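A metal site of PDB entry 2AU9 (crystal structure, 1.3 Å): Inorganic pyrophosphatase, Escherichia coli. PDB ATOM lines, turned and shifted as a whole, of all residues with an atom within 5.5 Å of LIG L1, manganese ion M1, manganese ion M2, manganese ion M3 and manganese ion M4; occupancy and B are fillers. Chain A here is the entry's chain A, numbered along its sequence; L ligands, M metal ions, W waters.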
ATOM      1  N   GLU A  20     -15.798  -8.611   7.862  1.00  0.00           N
ATOM      2  CA  GLU A  20     -14.662  -8.390   8.722  1.00  0.00           C
ATOM      3  C   GLU A  20     -14.354  -9.508   9.665  1.00  0.00           C
ATOM      4  O   GLU A  20     -13.184  -9.776   9.983  1.00  0.00           O
ATOM      5  CB  GLU A  20     -14.906  -7.131   9.608  1.00  0.00           C
ATOM      6  CG  GLU A  20     -14.947  -5.870   8.746  1.00  0.00           C
ATOM      7  CD  GLU A  20     -15.547  -4.667   9.461  1.00  0.00           C
ATOM      8  OE1 GLU A  20     -16.568  -4.869  10.116  1.00  0.00           O
ATOM      9  OE2 GLU A  20     -14.952  -3.554   9.287  1.00  0.00           O
ATOM     10  N   LYS A  29     -11.485  -8.854  16.937  1.00  0.00           N
ATOM     11  CA  LYS A  29     -12.434  -7.925  16.376  1.00  0.00           C
ATOM     12  C   LYS A  29     -11.748  -7.101  15.292  1.00  0.00           C
ATOM     13  O   LYS A  29     -11.209  -5.983  15.510  1.00  0.00           O
ATOM     14  CB  LYS A  29     -13.044  -7.017  17.473  1.00  0.00           C
ATOM     15  CG  LYS A  29     -14.457  -6.592  17.160  1.00  0.00           C
ATOM     16  CD  LYS A  29     -14.715  -5.574  16.107  1.00  0.00           C
ATOM     17  CE  LYS A  29     -16.152  -5.108  15.910  1.00  0.00           C
ATOM     18  NZ  LYS A  29     -16.366  -4.191  14.801  1.00  0.00           N
ATOM     19  N   GLU A  31     -11.550  -4.662  12.003  1.00  0.00           N
ATOM     20  CA  GLU A  31     -12.305  -3.591  11.336  1.00  0.00           C
ATOM     21  C   GLU A  31     -11.521  -3.136  10.139  1.00  0.00           C
ATOM     22  O   GLU A  31     -10.311  -2.856  10.259  1.00  0.00           O
ATOM     23  CB  GLU A  31     -12.619  -2.426  12.247  1.00  0.00           C
ATOM     24  CG  GLU A  31     -13.512  -2.823  13.358  1.00  0.00           C
ATOM     25  CD  GLU A  31     -13.958  -1.679  14.263  1.00  0.00           C
ATOM     26  OE1 GLU A  31     -13.542  -0.546  14.097  1.00  0.00           O
ATOM     27  OE2 GLU A  31     -14.775  -1.873  15.184  1.00  0.00           O
ATOM     28  N   ASP A  42      -9.129  -4.148  15.709  1.00  0.00           N
ATOM     29  CA  ASP A  42      -9.683  -3.103  16.562  1.00  0.00           C
ATOM     30  C   ASP A  42      -9.337  -3.434  18.009  1.00  0.00           C
ATOM     31  O   ASP A  42      -8.869  -2.583  18.828  1.00  0.00           O
ATOM     32  CB  ASP A  42     -11.175  -2.880  16.327  1.00  0.00           C
ATOM     33  CG  ASP A  42     -11.704  -1.867  17.324  1.00  0.00           C
ATOM     34  OD1 ASP A  42     -11.527  -0.649  17.087  1.00  0.00           O
ATOM     35  OD2 ASP A  42     -12.294  -2.182  18.353  1.00  0.00           O
ATOM     36  N   ARG A  43      -9.540  -4.711  18.393  1.00  0.00           N
ATOM     37  CA  ARG A  43      -9.311  -5.236  19.731  1.00  0.00           C
ATOM     38  C   ARG A  43      -9.447  -6.742  19.765  1.00  0.00           C
ATOM     39  O   ARG A  43      -9.994  -7.332  18.831  1.00  0.00           O
ATOM     40  CB  ARG A  43     -10.248  -4.628  20.803  1.00  0.00           C
ATOM     41  CG  ARG A  43     -11.688  -5.065  20.627  1.00  0.00           C
ATOM     42  CD  ARG A  43     -12.612  -4.162  21.491  1.00  0.00           C
ATOM     43  NE  ARG A  43     -14.014  -4.548  21.443  1.00  0.00           N
ATOM     44  CZ  ARG A  43     -14.945  -4.244  20.537  1.00  0.00           C
ATOM     45  NH1 ARG A  43     -14.619  -3.503  19.463  1.00  0.00           N
ATOM     46  NH2 ARG A  43     -16.208  -4.656  20.630  1.00  0.00           N
ATOM     47  N   TYR A  51     -19.198 -14.367  17.268  1.00  0.00           N
ATOM     48  CA  TYR A  51     -20.290 -13.818  16.451  1.00  0.00           C
ATOM     49  C   TYR A  51     -21.117 -14.953  15.892  1.00  0.00           C
ATOM     50  O   TYR A  51     -20.560 -15.929  15.339  1.00  0.00           O
ATOM     51  CB  TYR A  51     -19.777 -12.975  15.297  1.00  0.00           C
ATOM     52  CG  TYR A  51     -19.337 -11.616  15.725  1.00  0.00           C
ATOM     53  CD1 TYR A  51     -18.073 -11.399  16.306  1.00  0.00           C
ATOM     54  CD2 TYR A  51     -20.136 -10.488  15.631  1.00  0.00           C
ATOM     55  CE1 TYR A  51     -17.656 -10.132  16.733  1.00  0.00           C
ATOM     56  CE2 TYR A  51     -19.754  -9.232  16.032  1.00  0.00           C
ATOM     57  CZ  TYR A  51     -18.510  -9.070  16.578  1.00  0.00           C
ATOM     58  OH  TYR A  51     -18.067  -7.862  17.012  1.00  0.00           O
ATOM     59  N   TYR A  55     -19.816 -11.222  10.144  1.00  0.00           N
ATOM     60  CA  TYR A  55     -20.082  -9.847  10.510  1.00  0.00           C
ATOM     61  C   TYR A  55     -19.255  -8.889   9.668  1.00  0.00           C
ATOM     62  O   TYR A  55     -18.074  -9.078   9.471  1.00  0.00           O
ATOM     63  CB  TYR A  55     -19.717  -9.630  11.961  1.00  0.00           C
ATOM     64  CG  TYR A  55     -20.026  -8.275  12.551  1.00  0.00           C
ATOM     65  CD1 TYR A  55     -21.320  -7.952  12.898  1.00  0.00           C
ATOM     66  CD2 TYR A  55     -19.022  -7.338  12.721  1.00  0.00           C
ATOM     67  CE1 TYR A  55     -21.612  -6.720  13.408  1.00  0.00           C
ATOM     68  CE2 TYR A  55     -19.314  -6.074  13.264  1.00  0.00           C
ATOM     69  CZ  TYR A  55     -20.610  -5.788  13.608  1.00  0.00           C
ATOM     70  OH  TYR A  55     -20.934  -4.569  14.167  1.00  0.00           O
ATOM     71  N   GLY A  56     -19.921  -7.821   9.170  1.00  0.00           N
ATOM     72  CA  GLY A  56     -19.239  -6.797   8.457  1.00  0.00           C
ATOM     73  C   GLY A  56     -20.111  -5.555   8.224  1.00  0.00           C
ATOM     74  O   GLY A  56     -20.780  -5.138   9.170  1.00  0.00           O
ATOM     75  N   TYR A  57     -20.005  -5.009   6.998  1.00  0.00           N
ATOM     76  CA  TYR A  57     -20.669  -3.726   6.745  1.00  0.00           C
ATOM     77  C   TYR A  57     -21.020  -3.555   5.288  1.00  0.00           C
ATOM     78  O   TYR A  57     -20.493  -4.297   4.496  1.00  0.00           O
ATOM     79  CB  TYR A  57     -19.778  -2.593   7.297  1.00  0.00           C
ATOM     80  CG  TYR A  57     -18.509  -2.427   6.491  1.00  0.00           C
ATOM     81  CD1 TYR A  57     -17.401  -3.217   6.815  1.00  0.00           C
ATOM     82  CD2 TYR A  57     -18.345  -1.586   5.424  1.00  0.00           C
ATOM     83  CE1 TYR A  57     -16.216  -3.097   6.105  1.00  0.00           C
ATOM     84  CE2 TYR A  57     -17.163  -1.462   4.701  1.00  0.00           C
ATOM     85  CZ  TYR A  57     -16.088  -2.244   5.050  1.00  0.00           C
ATOM     86  OH  TYR A  57     -14.922  -2.188   4.385  1.00  0.00           O
ATOM     87  N   SER A  63     -23.531   4.929   9.687  1.00  0.00           N
ATOM     88  CA  SER A  63     -24.355   4.868  10.878  1.00  0.00           C
ATOM     89  C   SER A  63     -24.039   6.065  11.739  1.00  0.00           C
ATOM     90  O   SER A  63     -23.112   6.789  11.476  1.00  0.00           O
ATOM     91  CB  SER A  63     -23.957   3.598  11.618  1.00  0.00           C
ATOM     92  OG  SER A  63     -24.970   3.034  12.418  1.00  0.00           O
ATOM     93  N   ASP A  65     -22.920   5.752  14.604  1.00  0.00           N
ATOM     94  CA  ASP A  65     -21.732   5.466  15.426  1.00  0.00           C
ATOM     95  C   ASP A  65     -20.440   5.850  14.689  1.00  0.00           C
ATOM     96  O   ASP A  65     -19.340   5.569  15.178  1.00  0.00           O
ATOM     97  CB  ASP A  65     -21.690   4.019  15.861  1.00  0.00           C
ATOM     98  CG  ASP A  65     -21.315   3.047  14.760  1.00  0.00           C
ATOM     99  OD1 ASP A  65     -20.910   1.915  15.080  1.00  0.00           O
ATOM    100  OD2 ASP A  65     -21.497   3.422  13.592  1.00  0.00           O
ATOM    101  N   ASP A  67     -19.459   4.781  11.719  1.00  0.00           N
ATOM    102  CA  ASP A  67     -18.952   3.694  10.902  1.00  0.00           C
ATOM    103  C   ASP A  67     -19.994   3.313   9.865  1.00  0.00           C
ATOM    104  O   ASP A  67     -21.188   3.544  10.109  1.00  0.00           O
ATOM    105  CB  ASP A  67     -18.637   2.467  11.750  1.00  0.00           C
ATOM    106  CG  ASP A  67     -17.653   2.448  12.874  1.00  0.00           C
ATOM    107  OD1 ASP A  67     -16.806   3.365  12.863  1.00  0.00           O
ATOM    108  OD2 ASP A  67     -17.686   1.520  13.794  1.00  0.00           O
ATOM    109  N   PRO A  68     -19.630   2.660   8.758  1.00  0.00           N
ATOM    110  CA  PRO A  68     -20.669   2.051   7.871  1.00  0.00           C
ATOM    111  C   PRO A  68     -21.610   1.137   8.624  1.00  0.00           C
ATOM    112  O   PRO A  68     -21.278   0.529   9.626  1.00  0.00           O
ATOM    113  CB  PRO A  68     -19.828   1.277   6.854  1.00  0.00           C
ATOM    114  CG  PRO A  68     -18.475   1.922   6.848  1.00  0.00           C
ATOM    115  CD  PRO A  68     -18.259   2.454   8.217  1.00  0.00           C
ATOM    116  N   ASP A  70     -23.715  -1.885   9.974  1.00  0.00           N
ATOM    117  CA  ASP A  70     -23.296  -3.192  10.320  1.00  0.00           C
ATOM    118  C   ASP A  70     -24.279  -4.237   9.832  1.00  0.00           C
ATOM    119  O   ASP A  70     -25.526  -4.098   9.916  1.00  0.00           O
ATOM    120  CB  ASP A  70     -23.126  -3.360  11.834  1.00  0.00           C
ATOM    121  CG  ASP A  70     -22.109  -2.375  12.387  1.00  0.00           C
ATOM    122  OD1 ASP A  70     -21.071  -2.274  11.690  1.00  0.00           O
ATOM    123  OD2 ASP A  70     -22.326  -1.839  13.493  1.00  0.00           O
ATOM    124  N   MET A  95     -30.382  -1.377  18.123  1.00  0.00           N
ATOM    125  CA  MET A  95     -29.608  -1.274  19.355  1.00  0.00           C
ATOM    126  C   MET A  95     -28.766   0.004  19.311  1.00  0.00           C
ATOM    127  O   MET A  95     -28.463   0.636  18.285  1.00  0.00           O
ATOM    128  CB  MET A  95     -28.636  -2.425  19.623  1.00  0.00           C
ATOM    129  CG  MET A  95     -27.693  -2.681  18.429  1.00  0.00           C
ATOM    130  SD  MET A  95     -26.250  -3.700  18.865  1.00  0.00           S
ATOM    131  CE  MET A  95     -25.220  -2.387  19.508  1.00  0.00           C
ATOM    132  N   ASP A  97     -25.046   1.693  21.098  1.00  0.00           N
ATOM    133  CA  ASP A  97     -23.896   1.370  21.910  1.00  0.00           C
ATOM    134  C   ASP A  97     -23.161   2.674  22.186  1.00  0.00           C
ATOM    135  O   ASP A  97     -23.658   3.759  21.941  1.00  0.00           O
ATOM    136  CB  ASP A  97     -23.019   0.236  21.350  1.00  0.00           C
ATOM    137  CG  ASP A  97     -22.116   0.554  20.189  1.00  0.00           C
ATOM    138  OD1 ASP A  97     -21.904   1.701  19.734  1.00  0.00           O
ATOM    139  OD2 ASP A  97     -21.507  -0.464  19.733  1.00  0.00           O
ATOM    140  N   GLU A  98     -21.995   2.561  22.824  1.00  0.00           N
ATOM    141  CA  GLU A  98     -21.308   3.770  23.354  1.00  0.00           C
ATOM    142  C   GLU A  98     -20.959   4.727  22.250  1.00  0.00           C
ATOM    143  O   GLU A  98     -20.700   5.915  22.554  1.00  0.00           O
ATOM    144  CB  GLU A  98     -20.002   3.430  24.119  1.00  0.00           C
ATOM    145  CG  GLU A  98     -18.864   2.842  23.294  1.00  0.00           C
ATOM    146  CD  GLU A  98     -18.972   1.556  22.548  1.00  0.00           C
ATOM    147  OE1 GLU A  98     -19.753   0.715  23.037  1.00  0.00           O
ATOM    148  OE2 GLU A  98     -18.297   1.345  21.498  1.00  0.00           O
ATOM    149  N   ASP A 102     -26.751   2.105  16.550  1.00  0.00           N
ATOM    150  CA  ASP A 102     -25.879   1.173  15.893  1.00  0.00           C
ATOM    151  C   ASP A 102     -26.582  -0.110  15.526  1.00  0.00           C
ATOM    152  O   ASP A 102     -26.204  -1.217  15.972  1.00  0.00           O
ATOM    153  CB  ASP A 102     -24.737   0.912  16.916  1.00  0.00           C
ATOM    154  CG  ASP A 102     -23.535   0.195  16.317  1.00  0.00           C
ATOM    155  OD1 ASP A 102     -23.314   0.335  15.039  1.00  0.00           O
ATOM    156  OD2 ASP A 102     -22.803  -0.494  17.038  1.00  0.00           O
ATOM    157  N   LYS A 104     -28.041  -3.513  13.806  1.00  0.00           N
ATOM    158  CA  LYS A 104     -27.423  -4.705  13.265  1.00  0.00           C
ATOM    159  C   LYS A 104     -28.362  -5.302  12.230  1.00  0.00           C
ATOM    160  O   LYS A 104     -29.359  -5.951  12.538  1.00  0.00           O
ATOM    161  CB  LYS A 104     -27.082  -5.688  14.393  1.00  0.00           C
ATOM    162  CG  LYS A 104     -26.132  -5.126  15.430  1.00  0.00           C
ATOM    163  CD  LYS A 104     -24.720  -4.997  14.921  1.00  0.00           C
ATOM    164  CE  LYS A 104     -23.833  -4.322  15.916  1.00  0.00           C
ATOM    165  NZ  LYS A 104     -23.806  -2.868  15.680  1.00  0.00           N
ATOM    166  N   TYR A 141     -21.415  -9.127  24.923  1.00  0.00           N
ATOM    167  CA  TYR A 141     -20.044  -9.248  24.424  1.00  0.00           C
ATOM    168  C   TYR A 141     -19.132  -8.107  24.934  1.00  0.00           C
ATOM    169  O   TYR A 141     -17.900  -8.323  24.951  1.00  0.00           O
ATOM    170  CB  TYR A 141     -19.967  -9.339  22.895  1.00  0.00           C
ATOM    171  CG  TYR A 141     -20.114  -8.040  22.107  1.00  0.00           C
ATOM    172  CD1 TYR A 141     -21.227  -7.204  22.252  1.00  0.00           C
ATOM    173  CD2 TYR A 141     -19.107  -7.692  21.189  1.00  0.00           C
ATOM    174  CE1 TYR A 141     -21.328  -6.045  21.516  1.00  0.00           C
ATOM    175  CE2 TYR A 141     -19.226  -6.527  20.460  1.00  0.00           C
ATOM    176  CZ  TYR A 141     -20.339  -5.720  20.634  1.00  0.00           C
ATOM    177  OH  TYR A 141     -20.495  -4.530  19.935  1.00  0.00           O
ATOM    178  N   LYS A 142     -19.676  -6.968  25.353  1.00  0.00           N
ATOM    179  CA  LYS A 142     -18.960  -5.864  25.912  1.00  0.00           C
ATOM    180  C   LYS A 142     -18.960  -5.848  27.453  1.00  0.00           C
ATOM    181  O   LYS A 142     -18.502  -4.833  28.036  1.00  0.00           O
ATOM    182  CB  LYS A 142     -19.473  -4.496  25.356  1.00  0.00           C
ATOM    183  CG  LYS A 142     -19.101  -4.339  23.912  1.00  0.00           C
ATOM    184  CD  LYS A 142     -19.767  -3.153  23.223  1.00  0.00           C
ATOM    185  CE  LYS A 142     -19.000  -2.672  22.045  1.00  0.00           C
ATOM    186  NZ  LYS A 142     -19.640  -1.577  21.367  1.00  0.00           N
HETATM  187  P1  LIG L   1     -18.119  -2.670  18.009  1.00  0.00           P
HETATM  188  O1  LIG L   1     -19.005  -1.536  18.474  1.00  0.00           O
HETATM  189  O2  LIG L   1     -18.168  -4.023  18.667  1.00  0.00           O
HETATM  190  O3  LIG L   1     -16.677  -2.198  17.787  1.00  0.00           O
HETATM  191  O4  LIG L   1     -18.611  -2.958  16.452  1.00  0.00           O
HETATM  192  P2  LIG L   1     -18.940  -1.839  15.280  1.00  0.00           P
HETATM  193  O5  LIG L   1     -20.217  -1.174  15.682  1.00  0.00           O
HETATM  194  O6  LIG L   1     -19.084  -2.723  14.067  1.00  0.00           O
HETATM  195  O7  LIG L   1     -17.741  -1.065  15.311  1.00  0.00           O
HETATM  196  F1  LG2 L   2     -19.429  -0.075  13.182  1.00  0.00           F
HETATM  197 CL1  LG3 L   3     -21.605  -3.093  18.159  1.00  0.00          CL
HETATM  198 MN    MN M   1     -21.357  -0.036  14.163  1.00  0.00          MN
HETATM  199 MN    MN M   2     -18.969  -1.855  12.066  1.00  0.00          MN
HETATM  200 MN    MN M   3     -20.881  -0.910  17.730  1.00  0.00          MN
HETATM  201 MN    MN M   4     -16.015  -0.590  16.561  1.00  0.00          MN
HETATM  202  O   HOH W   1     -17.288   0.915  17.771  1.00  0.00           O
HETATM  203  O   HOH W   2     -16.826  -1.481  12.645  1.00  0.00           O
HETATM  204  O   HOH W   3     -16.613  -0.624  20.515  1.00  0.00           O
HETATM  205  O   HOH W   4     -14.397  -0.173  18.014  1.00  0.00           O
HETATM  206  O   HOH W   5     -19.815  -5.630  16.865  1.00  0.00           O
HETATM  207  O   HOH W   6     -18.781  -0.646  10.417  1.00  0.00           O
HETATM  208  O   HOH W   7     -22.052   0.986  12.370  1.00  0.00           O
HETATM  209  O   HOH W   8     -15.458   1.000  15.338  1.00  0.00           O
HETATM  210  O   HOH W   9     -20.264   1.214  17.579  1.00  0.00           O
HETATM  211  O   HOH W  10     -18.720  -3.642  10.927  1.00  0.00           O
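An oxygen (O6) of LIG L1 sits close to the side-chain hydroxyl (OH) of Tyr 55, at 2.6 Å.
The side-chain hydroxyl of Tyr 141 is in hydrogen-bond range of an oxygen (O2) of LIG L1, 2.7 Å away.
An oxygen (O2) of LIG L1 lies within salt-bridge range of the guanidinium group of Arg 43, at 2.8 Å.
The side-chain amino group (NZ) of Lys 142 lies within salt-bridge range of an oxygen (O2) of LIG L1 (3.9 Å).
An oxygen (O4) of LIG L1 lies within hydrogen-bond range of the side-chain amino group (NZ) of Lys 29.
An oxygen (O5) of LIG L1 sits close to the side-chain amino group (NZ) of Lys 104, at 3.97 Å.
O of Asp 102 lies within hydrogen-bond range of NZ of Lys 104 (2.9 Å).
The backbone NH of Asp 102 lies within hydrogen-bond range of the backbone carbonyl oxygen of Met 95, at 2.8 Å.
NZ of Lys 29 lies close to OE2 of Glu 31 (2.8 Å).
The backbone carbonyl oxygen (O) of Tyr 55 lies within hydrogen-bond range of the backbone NH (N) of Glu 20, 2.8 Å away.
The side-chain hydroxyl (OH) of Tyr 141 lies close to the side-chain amino group (NZ) of Lys 142.
O of Arg 43 lies within hydrogen-bond range of N of Lys 29 (2.9 Å).
The guanidinium group (NH1) of Arg 43 lies within salt-bridge range of the side-chain carboxylate (OD2) of Asp 42 (2.9 Å).
The side-chain amino group (NZ) of Lys 142 is in salt-bridge range of the side-chain carboxylate (OE1) of Glu 98, 2.8 Å away.
The side-chain carboxylate (OD2) of Asp 67 lies close to an oxygen (O7) of LIG L1, 3.0 Å away.
Hydrophobic or aromatic side chains that line LIG L1: Tyr 55 and Tyr 141.
Within 4 Å of LIG L1: Lys 29, Glu 31, Arg 43, Tyr 55, Asp 65, Asp 67, Asp 70, Asp 97, Asp 102, Lys 104, Tyr 141 and Lys 142.
The nearest printed residue that does not touch LIG L1 is Tyr 51 (4.2 Å).
The nearest printed residue that does not touch manganese ion M1 is Asp 67 (4.004 Å).
Tyr 55 touches manganese ion M2.
Two residues have an atom within 4 Å of manganese ion M2: Tyr 55 and Asp 70.
The nearest printed residue that does not touch manganese ion M2 is Asp 67 (4.003 Å).
Lys 142 touches manganese ion M3 (NZ to MN, 3.9 Å).
Of the 21 residues printed, 4 come within 4 Å of manganese ion M3.
OD2 of Asp 67 touches manganese ion M4, 3.9 Å away.
The side-chain carboxylate (OD2) of Asp 70 is bound to manganese ion M1, 2.2 Å away.
F1 of LG2 L2 is bound to manganese ion M1 (2.2 Å).
The side-chain carboxylate (OD1) of Asp 102 binds manganese ion M1 (2.2 Å).
Water W7 is bound to manganese ion M1 (2.2 Å).
OD1 of Asp 65 binds manganese ion M1, at 2.2 Å.
Manganese ion M1 is bound by an oxygen (O5) of LIG L1 (2.2 Å).
Manganese ion M1 has six donor atoms within binding distance.
Manganese ion M2 is bound by water W6 (2.1 Å), water W10 (2.1 Å), a fluorine (F1) of LG2 L2 (2.2 Å), the side-chain carboxylate of Asp 70 (2.2 Å), an oxygen (O6) of LIG L1 (2.2 Å) and water W2 (2.3 Å).
Manganese ion M2 has six donor atoms within binding distance.
Manganese ion M3 is bound by the side-chain carboxylate (OD2) of Asp 102, 2.1 Å away.
Manganese ion M3 is bound by O1 of LIG L1, 2.1 Å away.
OD2 of Asp 97 is bound to manganese ion M3 (2.1 Å).
Manganese ion M3 is bound by an oxygen (O5) of LIG L1, 2.2 Å away.
Water W9 is bound to manganese ion M3 (2.2 Å).
CL1 of LG3 L3 is bound to manganese ion M3, at 2.3 Å.
Manganese ion M4 is bound by water W8 (2.1 Å), O3 of LIG L1 (2.1 Å), O7 of LIG L1 (2.2 Å), water W4 (2.2 Å), OE2 of Glu 31 (2.3 Å) and water W1 (2.3 Å).
Water W7 lies within hydrogen-bond range of the side-chain carboxylate of Asp 65 (2.8 Å) and the backbone carbonyl oxygen of Pro 68 (2.9 Å).
Water W2 bridges OD2 of Asp 67 and NZ of Lys 29.
Water W10 lies within hydrogen-bond range of the side-chain carboxylate of Glu 20 (2.6 Å) and the backbone carbonyl oxygen of Gly 56 (3.1 Å).
Water W8 lies within hydrogen-bond range of OE1 of Glu 31 (2.8 Å) and OD2 of Asp 67 (2.8 Å).
Water W5 lies within hydrogen-bond range of the side-chain hydroxyl (OH) of Tyr 51 (2.8 Å), an oxygen (O2) of LIG L1 (2.9 Å), the side-chain hydroxyl (OH) of Tyr 55 (3.1 Å) and the side-chain hydroxyl (OH) of Tyr 141 (3.3 Å).
Water W3 lies within hydrogen-bond range of OE2 of Glu 98 and NZ of Lys 142.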
